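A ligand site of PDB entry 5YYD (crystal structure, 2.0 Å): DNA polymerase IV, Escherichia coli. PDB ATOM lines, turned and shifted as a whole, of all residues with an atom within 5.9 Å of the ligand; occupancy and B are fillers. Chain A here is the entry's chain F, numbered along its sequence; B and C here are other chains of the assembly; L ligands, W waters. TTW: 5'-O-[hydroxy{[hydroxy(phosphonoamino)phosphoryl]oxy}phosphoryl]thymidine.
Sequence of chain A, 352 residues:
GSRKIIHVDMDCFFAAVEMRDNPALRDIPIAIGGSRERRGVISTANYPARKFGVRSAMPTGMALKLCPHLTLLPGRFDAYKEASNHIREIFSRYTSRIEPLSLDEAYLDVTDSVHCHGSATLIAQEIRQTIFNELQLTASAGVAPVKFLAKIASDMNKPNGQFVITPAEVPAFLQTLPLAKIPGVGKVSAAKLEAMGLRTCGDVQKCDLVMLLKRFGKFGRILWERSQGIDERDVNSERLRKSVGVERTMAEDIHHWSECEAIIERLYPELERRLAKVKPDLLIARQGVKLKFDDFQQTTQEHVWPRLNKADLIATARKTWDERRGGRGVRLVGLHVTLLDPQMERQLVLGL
O of Met 10 lies close to O2B of the ligand (3.3 Å). OD2 of Asp 104 lies close to O2A of the ligand, at 3.4 Å. An oxygen (O2A) of the ligand sits close to the side-chain carboxylate (OE1) of Glu 105, 3.4 Å away. O3' of DC 18 of chain C sits close to an oxygen (O5') of the ligand (3.3 Å). Asp 9 touches the ligand (OD1 to O2A, 3.5 Å). CA of Asp 11 touches O1G of the ligand, at 3.3 Å. Ser 56 touches the ligand (CB to C5M, 3.8 Å). DG 5 of chain B touches the ligand (N2 to O2, 3.6 Å).
The side-chain hydroxyl (OG1) of Thr 44 lies within hydrogen-bond range of the guanidinium group (NH2) of Arg 50, at 3.1 Å. SG of Cys 12 lies within hydrogen-bond range of O of Ala 45 (3.5 Å). OG of Ser 56 sits at hydrogen-bond distance from O of Ser 43. The backbone carbonyl oxygen (O) of Ala 45 is in hydrogen-bond range of the guanidinium group (NE) of Arg 50 (3.0 Å). The side-chain hydroxyl of Ser 102 sits at hydrogen-bond distance from O3' of DC 18 of chain C (2.8 Å). The side-chain amino group (NZ) of Lys 158 lies within salt-bridge range of the side-chain carboxylate (OD1) of Asp 155 (3.4 Å). The backbone carbonyl oxygen (O) of Asp 104 is in hydrogen-bond range of the backbone NH (N) of Met 10. The side-chain carboxylate (OD1) of Asp 104 is in hydrogen-bond range of the side-chain hydroxyl (OG) of Ser 102, 3.2 Å away.
The side-chain hydroxyl of Thr 44 is in hydrogen-bond range of an oxygen (O1B) of the ligand, at 2.6 Å. The backbone NH (N) of Cys 12 is in hydrogen-bond range of an oxygen (O1G) of the ligand (2.8 Å). N1 of DA 4 of chain B sits at hydrogen-bond distance from a nitrogen (N3) of the ligand, 2.9 Å away. O of Ser 43 lies close to N3 of the ligand. An oxygen (O2) of the ligand sits at hydrogen-bond distance from the side-chain hydroxyl of Ser 43, 2.9 Å away. The backbone NH of Phe 13 lies within hydrogen-bond range of an oxygen (O2B) of the ligand. An oxygen (O1B) of the ligand is in salt-bridge range of the guanidinium group (NH2) of Arg 50, 3.6 Å away. NZ of Lys 158 lies within salt-bridge range of O2G of the ligand. N of Phe 14 is in hydrogen-bond range of O3' of the ligand (3.3 Å).
Water W4 lies within hydrogen-bond range of O1G of the ligand, OH of Tyr 47 and OD1 of Asp 11. Water W5 lies within hydrogen-bond range of O1A of the ligand and OP2 of DC 18 of chain C. Water W6 bridges an oxygen (O3G) of the ligand (2.9 Å) and the guanidinium group of Arg 50 (3.2 Å). Water W2 lies within hydrogen-bond range of OG of Ser 56 (2.7 Å), NH2 of Arg 50 (2.8 Å) and O3A of the ligand (3.5 Å). Water W7 bridges N of Asp 104 (2.9 Å) and O3' of DC 18 of chain C (3.3 Å).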
ATOM      1  N   ASP A   9     -16.004  -1.915 -21.797  1.00  0.00           N
ATOM      2  CA  ASP A   9     -16.529  -0.777 -21.052  1.00  0.00           C
ATOM      3  C   ASP A   9     -17.195  -1.256 -19.768  1.00  0.00           C
ATOM      4  O   ASP A   9     -18.193  -1.972 -19.842  1.00  0.00           O
ATOM      5  CB  ASP A   9     -17.532  -0.007 -21.918  1.00  0.00           C
ATOM      6  CG  ASP A   9     -17.854   1.367 -21.354  1.00  0.00           C
ATOM      7  OD1 ASP A   9     -17.863   1.508 -20.130  1.00  0.00           O
ATOM      8  OD2 ASP A   9     -18.106   2.298 -22.149  1.00  0.00           O
ATOM      9  N   MET A  10     -16.664  -0.822 -18.605  1.00  0.00           N
ATOM     10  CA  MET A  10     -17.185  -1.272 -17.318  1.00  0.00           C
ATOM     11  C   MET A  10     -18.584  -0.724 -17.078  1.00  0.00           C
ATOM     12  O   MET A  10     -18.895   0.404 -17.453  1.00  0.00           O
ATOM     13  CB  MET A  10     -16.261  -0.850 -16.168  1.00  0.00           C
ATOM     14  CG  MET A  10     -14.872  -1.424 -16.238  1.00  0.00           C
ATOM     15  SD  MET A  10     -14.790  -3.235 -16.303  1.00  0.00           S
ATOM     16  CE  MET A  10     -15.108  -3.655 -14.593  1.00  0.00           C
ATOM     17  N   ASP A  11     -19.431  -1.529 -16.422  1.00  0.00           N
ATOM     18  CA  ASP A  11     -20.799  -1.107 -16.131  1.00  0.00           C
ATOM     19  C   ASP A  11     -20.830  -0.241 -14.872  1.00  0.00           C
ATOM     20  O   ASP A  11     -20.280  -0.623 -13.842  1.00  0.00           O
ATOM     21  CB  ASP A  11     -21.701  -2.338 -15.934  1.00  0.00           C
ATOM     22  CG  ASP A  11     -21.765  -3.249 -17.168  1.00  0.00           C
ATOM     23  OD1 ASP A  11     -21.958  -2.736 -18.288  1.00  0.00           O
ATOM     24  OD2 ASP A  11     -21.629  -4.472 -17.000  1.00  0.00           O
ATOM     25  N   CYS A  12     -21.499   0.923 -14.968  1.00  0.00           N
ATOM     26  CA  CYS A  12     -21.664   1.869 -13.861  1.00  0.00           C
ATOM     27  C   CYS A  12     -20.433   1.915 -12.959  1.00  0.00           C
ATOM     28  O   CYS A  12     -20.502   1.688 -11.747  1.00  0.00           O
ATOM     29  CB  CYS A  12     -22.914   1.513 -13.038  1.00  0.00           C
ATOM     30  SG  CYS A  12     -24.427   1.590 -14.037  1.00  0.00           S
ATOM     31  N   PHE A  13     -19.280   2.224 -13.587  1.00  0.00           N
ATOM     32  CA  PHE A  13     -17.993   1.844 -13.015  1.00  0.00           C
ATOM     33  C   PHE A  13     -17.849   2.248 -11.536  1.00  0.00           C
ATOM     34  O   PHE A  13     -17.673   1.374 -10.676  1.00  0.00           O
ATOM     35  CB  PHE A  13     -16.847   2.425 -13.850  1.00  0.00           C
ATOM     36  CG  PHE A  13     -15.497   2.025 -13.360  1.00  0.00           C
ATOM     37  CD1 PHE A  13     -15.230   0.712 -13.005  1.00  0.00           C
ATOM     38  CD2 PHE A  13     -14.478   2.977 -13.227  1.00  0.00           C
ATOM     39  CE1 PHE A  13     -13.988   0.339 -12.540  1.00  0.00           C
ATOM     40  CE2 PHE A  13     -13.249   2.621 -12.783  1.00  0.00           C
ATOM     41  CZ  PHE A  13     -12.990   1.307 -12.423  1.00  0.00           C
ATOM     42  N   PHE A  14     -17.914   3.548 -11.219  1.00  0.00           N
ATOM     43  CA  PHE A  14     -17.675   3.939  -9.823  1.00  0.00           C
ATOM     44  C   PHE A  14     -18.685   3.271  -8.900  1.00  0.00           C
ATOM     45  O   PHE A  14     -18.327   2.739  -7.841  1.00  0.00           O
ATOM     46  CB  PHE A  14     -17.737   5.459  -9.618  1.00  0.00           C
ATOM     47  CG  PHE A  14     -16.651   6.217 -10.261  1.00  0.00           C
ATOM     48  CD1 PHE A  14     -15.699   5.593 -11.035  1.00  0.00           C
ATOM     49  CD2 PHE A  14     -16.579   7.591 -10.098  1.00  0.00           C
ATOM     50  CE1 PHE A  14     -14.700   6.329 -11.655  1.00  0.00           C
ATOM     51  CE2 PHE A  14     -15.577   8.332 -10.688  1.00  0.00           C
ATOM     52  CZ  PHE A  14     -14.653   7.708 -11.473  1.00  0.00           C
ATOM     53  N   ALA A  15     -19.961   3.322  -9.272  1.00  0.00           N
ATOM     54  CA  ALA A  15     -21.023   2.734  -8.453  1.00  0.00           C
ATOM     55  C   ALA A  15     -20.862   1.221  -8.332  1.00  0.00           C
ATOM     56  O   ALA A  15     -21.039   0.669  -7.239  1.00  0.00           O
ATOM     57  CB  ALA A  15     -22.391   3.098  -9.031  1.00  0.00           C
ATOM     58  N   ILE A  42     -23.671  14.646 -10.205  1.00  0.00           N
ATOM     59  CA  ILE A  42     -23.548  13.195 -10.166  1.00  0.00           C
ATOM     60  C   ILE A  42     -22.406  12.786 -11.087  1.00  0.00           C
ATOM     61  O   ILE A  42     -22.393  13.137 -12.265  1.00  0.00           O
ATOM     62  CB  ILE A  42     -24.847  12.509 -10.596  1.00  0.00           C
ATOM     63  CG1 ILE A  42     -26.025  12.926  -9.676  1.00  0.00           C
ATOM     64  CG2 ILE A  42     -24.641  10.984 -10.655  1.00  0.00           C
ATOM     65  CD1 ILE A  42     -25.780  12.613  -8.231  1.00  0.00           C
ATOM     66  N   SER A  43     -21.434  12.038 -10.539  1.00  0.00           N
ATOM     67  CA  SER A  43     -20.420  11.416 -11.392  1.00  0.00           C
ATOM     68  C   SER A  43     -20.998  10.205 -12.119  1.00  0.00           C
ATOM     69  O   SER A  43     -20.845  10.049 -13.331  1.00  0.00           O
ATOM     70  CB  SER A  43     -19.190  10.994 -10.590  1.00  0.00           C
ATOM     71  OG  SER A  43     -18.187  11.993 -10.651  1.00  0.00           O
ATOM     72  N   THR A  44     -21.612   9.311 -11.366  1.00  0.00           N
ATOM     73  CA  THR A  44     -22.395   8.221 -11.954  1.00  0.00           C
ATOM     74  C   THR A  44     -23.334   7.694 -10.879  1.00  0.00           C
ATOM     75  O   THR A  44     -23.297   8.133  -9.732  1.00  0.00           O
ATOM     76  CB  THR A  44     -21.496   7.114 -12.496  1.00  0.00           C
ATOM     77  OG1 THR A  44     -22.315   6.204 -13.217  1.00  0.00           O
ATOM     78  CG2 THR A  44     -20.864   6.362 -11.356  1.00  0.00           C
ATOM     79  N   ALA A  45     -24.170   6.732 -11.276  1.00  0.00           N
ATOM     80  CA  ALA A  45     -25.185   6.182 -10.399  1.00  0.00           C
ATOM     81  C   ALA A  45     -25.419   4.719 -10.745  1.00  0.00           C
ATOM     82  O   ALA A  45     -25.082   4.250 -11.836  1.00  0.00           O
ATOM     83  CB  ALA A  45     -26.486   6.982 -10.517  1.00  0.00           C
ATOM     84  N   TYR A  47     -28.112   1.287 -11.090  1.00  0.00           N
ATOM     85  CA  TYR A  47     -29.356   1.125 -11.849  1.00  0.00           C
ATOM     86  C   TYR A  47     -30.600   1.441 -10.995  1.00  0.00           C
ATOM     87  O   TYR A  47     -31.536   2.070 -11.504  1.00  0.00           O
ATOM     88  CB  TYR A  47     -29.418  -0.281 -12.484  1.00  0.00           C
ATOM     89  CG  TYR A  47     -28.729  -0.308 -13.856  1.00  0.00           C
ATOM     90  CD1 TYR A  47     -29.299   0.316 -14.951  1.00  0.00           C
ATOM     91  CD2 TYR A  47     -27.480  -0.906 -14.028  1.00  0.00           C
ATOM     92  CE1 TYR A  47     -28.662   0.345 -16.190  1.00  0.00           C
ATOM     93  CE2 TYR A  47     -26.850  -0.892 -15.260  1.00  0.00           C
ATOM     94  CZ  TYR A  47     -27.444  -0.263 -16.336  1.00  0.00           C
ATOM     95  OH  TYR A  47     -26.840  -0.240 -17.574  1.00  0.00           O
ATOM     96  N   ARG A  50     -30.706   5.205 -11.483  1.00  0.00           N
ATOM     97  CA  ARG A  50     -31.058   5.548 -12.866  1.00  0.00           C
ATOM     98  C   ARG A  50     -32.529   5.309 -13.162  1.00  0.00           C
ATOM     99  O   ARG A  50     -33.121   5.988 -14.001  1.00  0.00           O
ATOM    100  CB  ARG A  50     -30.206   4.727 -13.862  1.00  0.00           C
ATOM    101  CG  ARG A  50     -28.729   5.052 -13.771  1.00  0.00           C
ATOM    102  CD  ARG A  50     -27.824   4.114 -14.608  1.00  0.00           C
ATOM    103  NE  ARG A  50     -26.466   4.635 -14.501  1.00  0.00           N
ATOM    104  CZ  ARG A  50     -25.586   4.676 -15.485  1.00  0.00           C
ATOM    105  NH1 ARG A  50     -25.901   4.193 -16.679  1.00  0.00           N
ATOM    106  NH2 ARG A  50     -24.373   5.178 -15.247  1.00  0.00           N
ATOM    107  N   SER A  56     -25.379  10.749 -15.036  1.00  0.00           N
ATOM    108  CA  SER A  56     -24.120  11.480 -14.957  1.00  0.00           C
ATOM    109  C   SER A  56     -24.276  12.906 -15.462  1.00  0.00           C
ATOM    110  O   SER A  56     -25.065  13.184 -16.369  1.00  0.00           O
ATOM    111  CB  SER A  56     -23.034  10.775 -15.779  1.00  0.00           C
ATOM    112  OG  SER A  56     -22.656   9.540 -15.190  1.00  0.00           O
ATOM    113  N   ALA A  57     -23.532  13.834 -14.837  1.00  0.00           N
ATOM    114  CA  ALA A  57     -23.481  15.255 -15.162  1.00  0.00           C
ATOM    115  C   ALA A  57     -24.733  15.986 -14.656  1.00  0.00           C
ATOM    116  O   ALA A  57     -24.888  17.195 -14.908  1.00  0.00           O
ATOM    117  CB  ALA A  57     -23.294  15.537 -16.659  1.00  0.00           C
ATOM    118  N   SER A 102      -9.938   5.882 -20.691  1.00  0.00           N
ATOM    119  CA  SER A 102     -10.317   6.389 -19.387  1.00  0.00           C
ATOM    120  C   SER A 102     -10.019   5.252 -18.444  1.00  0.00           C
ATOM    121  O   SER A 102      -9.548   4.202 -18.900  1.00  0.00           O
ATOM    122  CB  SER A 102     -11.789   6.803 -19.364  1.00  0.00           C
ATOM    123  OG  SER A 102     -12.655   5.700 -19.613  1.00  0.00           O
ATOM    124  N   ASP A 104     -12.061   3.181 -17.095  1.00  0.00           N
ATOM    125  CA  ASP A 104     -12.971   2.046 -17.172  1.00  0.00           C
ATOM    126  C   ASP A 104     -13.157   1.503 -18.592  1.00  0.00           C
ATOM    127  O   ASP A 104     -14.032   0.651 -18.793  1.00  0.00           O
ATOM    128  CB  ASP A 104     -14.319   2.416 -16.550  1.00  0.00           C
ATOM    129  CG  ASP A 104     -15.310   2.962 -17.559  1.00  0.00           C
ATOM    130  OD1 ASP A 104     -14.927   3.765 -18.453  1.00  0.00           O
ATOM    131  OD2 ASP A 104     -16.509   2.583 -17.454  1.00  0.00           O
ATOM    132  N   GLU A 105     -12.391   1.971 -19.578  1.00  0.00           N
ATOM    133  CA  GLU A 105     -12.652   1.495 -20.928  1.00  0.00           C
ATOM    134  C   GLU A 105     -11.405   1.582 -21.805  1.00  0.00           C
ATOM    135  O   GLU A 105     -10.443   2.318 -21.509  1.00  0.00           O
ATOM    136  CB  GLU A 105     -13.848   2.226 -21.564  1.00  0.00           C
ATOM    137  CG  GLU A 105     -13.770   3.717 -21.709  1.00  0.00           C
ATOM    138  CD  GLU A 105     -15.153   4.362 -22.026  1.00  0.00           C
ATOM    139  OE1 GLU A 105     -15.994   4.569 -21.098  1.00  0.00           O
ATOM    140  OE2 GLU A 105     -15.360   4.705 -23.215  1.00  0.00           O
ATOM    141  N   ASP A 155     -22.554  -0.121 -25.936  1.00  0.00           N
ATOM    142  CA  ASP A 155     -23.712   0.412 -25.234  1.00  0.00           C
ATOM    143  C   ASP A 155     -25.012  -0.338 -25.529  1.00  0.00           C
ATOM    144  O   ASP A 155     -26.002  -0.113 -24.821  1.00  0.00           O
ATOM    145  CB  ASP A 155     -23.931   1.885 -25.607  1.00  0.00           C
ATOM    146  CG  ASP A 155     -22.910   2.778 -24.981  1.00  0.00           C
ATOM    147  OD1 ASP A 155     -22.371   2.374 -23.933  1.00  0.00           O
ATOM    148  OD2 ASP A 155     -22.632   3.861 -25.546  1.00  0.00           O
ATOM    149  N   LYS A 158     -25.841  -3.424 -22.773  1.00  0.00           N
ATOM    150  CA  LYS A 158     -25.285  -3.234 -21.451  1.00  0.00           C
ATOM    151  C   LYS A 158     -26.457  -3.193 -20.462  1.00  0.00           C
ATOM    152  O   LYS A 158     -27.551  -2.803 -20.835  1.00  0.00           O
ATOM    153  CB  LYS A 158     -24.397  -1.977 -21.406  1.00  0.00           C
ATOM    154  CG  LYS A 158     -25.140  -0.679 -21.349  1.00  0.00           C
ATOM    155  CD  LYS A 158     -24.230   0.536 -21.578  1.00  0.00           C
ATOM    156  CE  LYS A 158     -22.929   0.522 -20.753  1.00  0.00           C
ATOM    157  NZ  LYS A 158     -21.729   0.098 -21.523  1.00  0.00           N
ATOM    158  P    DA B   4     -20.606  22.452 -11.808  1.00  0.00           P
ATOM    159  OP1  DA B   4     -20.445  23.752 -11.120  1.00  0.00           O
ATOM    160  OP2  DA B   4     -20.316  22.442 -13.246  1.00  0.00           O
ATOM    161  O5'  DA B   4     -19.810  21.303 -11.113  1.00  0.00           O
ATOM    162  C5'  DA B   4     -19.959  21.003  -9.767  1.00  0.00           C
ATOM    163  C4'  DA B   4     -18.796  20.157  -9.315  1.00  0.00           C
ATOM    164  O4'  DA B   4     -18.799  18.851 -10.007  1.00  0.00           O
ATOM    165  C3'  DA B   4     -17.428  20.757  -9.606  1.00  0.00           C
ATOM    166  O3'  DA B   4     -16.543  20.404  -8.578  1.00  0.00           O
ATOM    167  C2'  DA B   4     -17.020  20.106 -10.958  1.00  0.00           C
ATOM    168  C1'  DA B   4     -17.704  18.748 -10.897  1.00  0.00           C
ATOM    169  N9   DA B   4     -18.235  18.271 -12.179  1.00  0.00           N
ATOM    170  C8   DA B   4     -18.877  19.006 -13.143  1.00  0.00           C
ATOM    171  N7   DA B   4     -19.305  18.282 -14.158  1.00  0.00           N
ATOM    172  C5   DA B   4     -18.949  16.999 -13.821  1.00  0.00           C
ATOM    173  C6   DA B   4     -19.115  15.766 -14.480  1.00  0.00           C
ATOM    174  N6   DA B   4     -19.713  15.642 -15.668  1.00  0.00           N
ATOM    175  N1   DA B   4     -18.651  14.666 -13.866  1.00  0.00           N
ATOM    176  C2   DA B   4     -18.041  14.807 -12.672  1.00  0.00           C
ATOM    177  N3   DA B   4     -17.829  15.918 -11.953  1.00  0.00           N
ATOM    178  C4   DA B   4     -18.301  16.977 -12.595  1.00  0.00           C
ATOM    179  P    DG B   5     -15.069  21.025  -8.549  1.00  0.00           P
ATOM    180  OP1  DG B   5     -14.703  21.119  -7.114  1.00  0.00           O
ATOM    181  OP2  DG B   5     -15.053  22.177  -9.450  1.00  0.00           O
ATOM    182  O5'  DG B   5     -14.173  19.926  -9.268  1.00  0.00           O
ATOM    183  C5'  DG B   5     -13.939  18.692  -8.673  1.00  0.00           C
ATOM    184  C4'  DG B   5     -13.135  17.846  -9.616  1.00  0.00           C
ATOM    185  O4'  DG B   5     -13.971  17.451 -10.742  1.00  0.00           O
ATOM    186  C3'  DG B   5     -11.919  18.569 -10.211  1.00  0.00           C
ATOM    187  O3'  DG B   5     -10.834  17.698 -10.157  1.00  0.00           O
ATOM    188  C2'  DG B   5     -12.343  18.862 -11.660  1.00  0.00           C
ATOM    189  C1'  DG B   5     -13.256  17.675 -11.932  1.00  0.00           C
ATOM    190  N9   DG B   5     -14.177  17.831 -13.037  1.00  0.00           N
ATOM    191  C8   DG B   5     -14.765  18.982 -13.506  1.00  0.00           C
ATOM    192  N7   DG B   5     -15.572  18.780 -14.526  1.00  0.00           N
ATOM    193  C5   DG B   5     -15.487  17.406 -14.758  1.00  0.00           C
ATOM    194  C6   DG B   5     -16.112  16.603 -15.757  1.00  0.00           C
ATOM    195  O6   DG B   5     -16.899  16.941 -16.645  1.00  0.00           O
ATOM    196  N1   DG B   5     -15.769  15.258 -15.616  1.00  0.00           N
ATOM    197  C2   DG B   5     -14.925  14.764 -14.659  1.00  0.00           C
ATOM    198  N2   DG B   5     -14.697  13.435 -14.690  1.00  0.00           N
ATOM    199  N3   DG B   5     -14.338  15.509 -13.725  1.00  0.00           N
ATOM    200  C4   DG B   5     -14.653  16.811 -13.847  1.00  0.00           C
ATOM    201  P    DC C  18     -16.550   8.717 -23.826  1.00  0.00           P
ATOM    202  OP1  DC C  18     -15.654   7.700 -24.394  1.00  0.00           O
ATOM    203  OP2  DC C  18     -18.034   8.645 -23.910  1.00  0.00           O
ATOM    204  O5'  DC C  18     -16.159   8.807 -22.282  1.00  0.00           O
ATOM    205  C5'  DC C  18     -14.820   8.631 -21.906  1.00  0.00           C
ATOM    206  C4'  DC C  18     -14.676   8.746 -20.414  1.00  0.00           C
ATOM    207  O4'  DC C  18     -14.886  10.128 -20.027  1.00  0.00           O
ATOM    208  C3'  DC C  18     -15.675   7.898 -19.626  1.00  0.00           C
ATOM    209  O3'  DC C  18     -14.989   6.967 -18.803  1.00  0.00           O
ATOM    210  C2'  DC C  18     -16.459   8.934 -18.773  1.00  0.00           C
ATOM    211  C1'  DC C  18     -15.542  10.153 -18.790  1.00  0.00           C
ATOM    212  N1   DC C  18     -16.247  11.448 -18.703  1.00  0.00           N
ATOM    213  C2   DC C  18     -15.976  12.270 -17.639  1.00  0.00           C
ATOM    214  O2   DC C  18     -15.196  11.856 -16.763  1.00  0.00           O
ATOM    215  N3   DC C  18     -16.579  13.473 -17.575  1.00  0.00           N
ATOM    216  C4   DC C  18     -17.402  13.868 -18.538  1.00  0.00           C
ATOM    217  N4   DC C  18     -17.966  15.056 -18.425  1.00  0.00           N
ATOM    218  C5   DC C  18     -17.705  13.013 -19.651  1.00  0.00           C
ATOM    219  C6   DC C  18     -17.097  11.834 -19.699  1.00  0.00           C
HETATM  220  O4  TTW L   1     -19.894  12.764 -16.670  1.00  0.00           O
HETATM  221  C4  TTW L   1     -19.203  11.742 -16.078  1.00  0.00           C
HETATM  222  N3  TTW L   1     -18.544  11.985 -14.961  1.00  0.00           N
HETATM  223  C2  TTW L   1     -17.856  11.029 -14.359  1.00  0.00           C
HETATM  224  O2  TTW L   1     -17.290  11.300 -13.347  1.00  0.00           O
HETATM  225  C5  TTW L   1     -19.204  10.499 -16.664  1.00  0.00           C
HETATM  226  C5M TTW L   1     -20.033  10.285 -17.992  1.00  0.00           C
HETATM  227  C6  TTW L   1     -18.473   9.521 -16.005  1.00  0.00           C
HETATM  228  N1  TTW L   1     -17.803   9.804 -14.879  1.00  0.00           N
HETATM  229  C1' TTW L   1     -17.057   8.765 -14.207  1.00  0.00           C
HETATM  230  O4' TTW L   1     -16.401   7.791 -15.315  1.00  0.00           O
HETATM  231  C2' TTW L   1     -17.850   7.988 -13.462  1.00  0.00           C
HETATM  232  C3' TTW L   1     -18.237   6.783 -14.388  1.00  0.00           C
HETATM  233  O3' TTW L   1     -18.569   5.654 -13.699  1.00  0.00           O
HETATM  234  C4' TTW L   1     -16.852   6.574 -15.118  1.00  0.00           C
HETATM  235  C5' TTW L   1     -17.020   5.803 -16.475  1.00  0.00           C
HETATM  236  O5' TTW L   1     -17.901   6.608 -17.248  1.00  0.00           O
HETATM  237  PA  TTW L   1     -19.059   5.965 -18.228  1.00  0.00           P
HETATM  238  O1A TTW L   1     -19.565   6.980 -19.253  1.00  0.00           O
HETATM  239  O2A TTW L   1     -18.635   4.715 -18.956  1.00  0.00           O
HETATM  240  O3A TTW L   1     -20.419   5.683 -17.335  1.00  0.00           O
HETATM  241  PB  TTW L   1     -20.675   4.427 -16.311  1.00  0.00           P
HETATM  242  O1B TTW L   1     -20.839   4.950 -14.916  1.00  0.00           O
HETATM  243  O2B TTW L   1     -19.571   3.407 -16.259  1.00  0.00           O
HETATM  244  N3B TTW L   1     -22.137   3.748 -16.791  1.00  0.00           N
HETATM  245  PG  TTW L   1     -22.207   2.749 -18.148  1.00  0.00           P
HETATM  246  O1G TTW L   1     -22.481   1.355 -17.591  1.00  0.00           O
HETATM  247  O2G TTW L   1     -20.906   2.778 -18.935  1.00  0.00           O
HETATM  248  O3G TTW L   1     -23.334   3.264 -19.012  1.00  0.00           O
HETATM  249  O   HOH W   1     -22.119   7.611 -19.491  1.00  0.00           O
HETATM  250  O   HOH W   2     -23.378   7.399 -16.676  1.00  0.00           O
HETATM  251  O   HOH W   3     -21.218  13.480 -19.025  1.00  0.00           O
HETATM  252  O   HOH W   4     -24.156  -0.570 -17.334  1.00  0.00           O
HETATM  253  O   HOH W   5     -19.087   8.955 -21.066  1.00  0.00           O
HETATM  254  O   HOH W   6     -24.565   5.854 -19.062  1.00  0.00           O
HETATM  255  O   HOH W   7     -13.560   5.504 -16.196  1.00  0.00           O
HETATM  256  O   HOH W   8     -14.105  10.222 -14.876  1.00  0.00           O
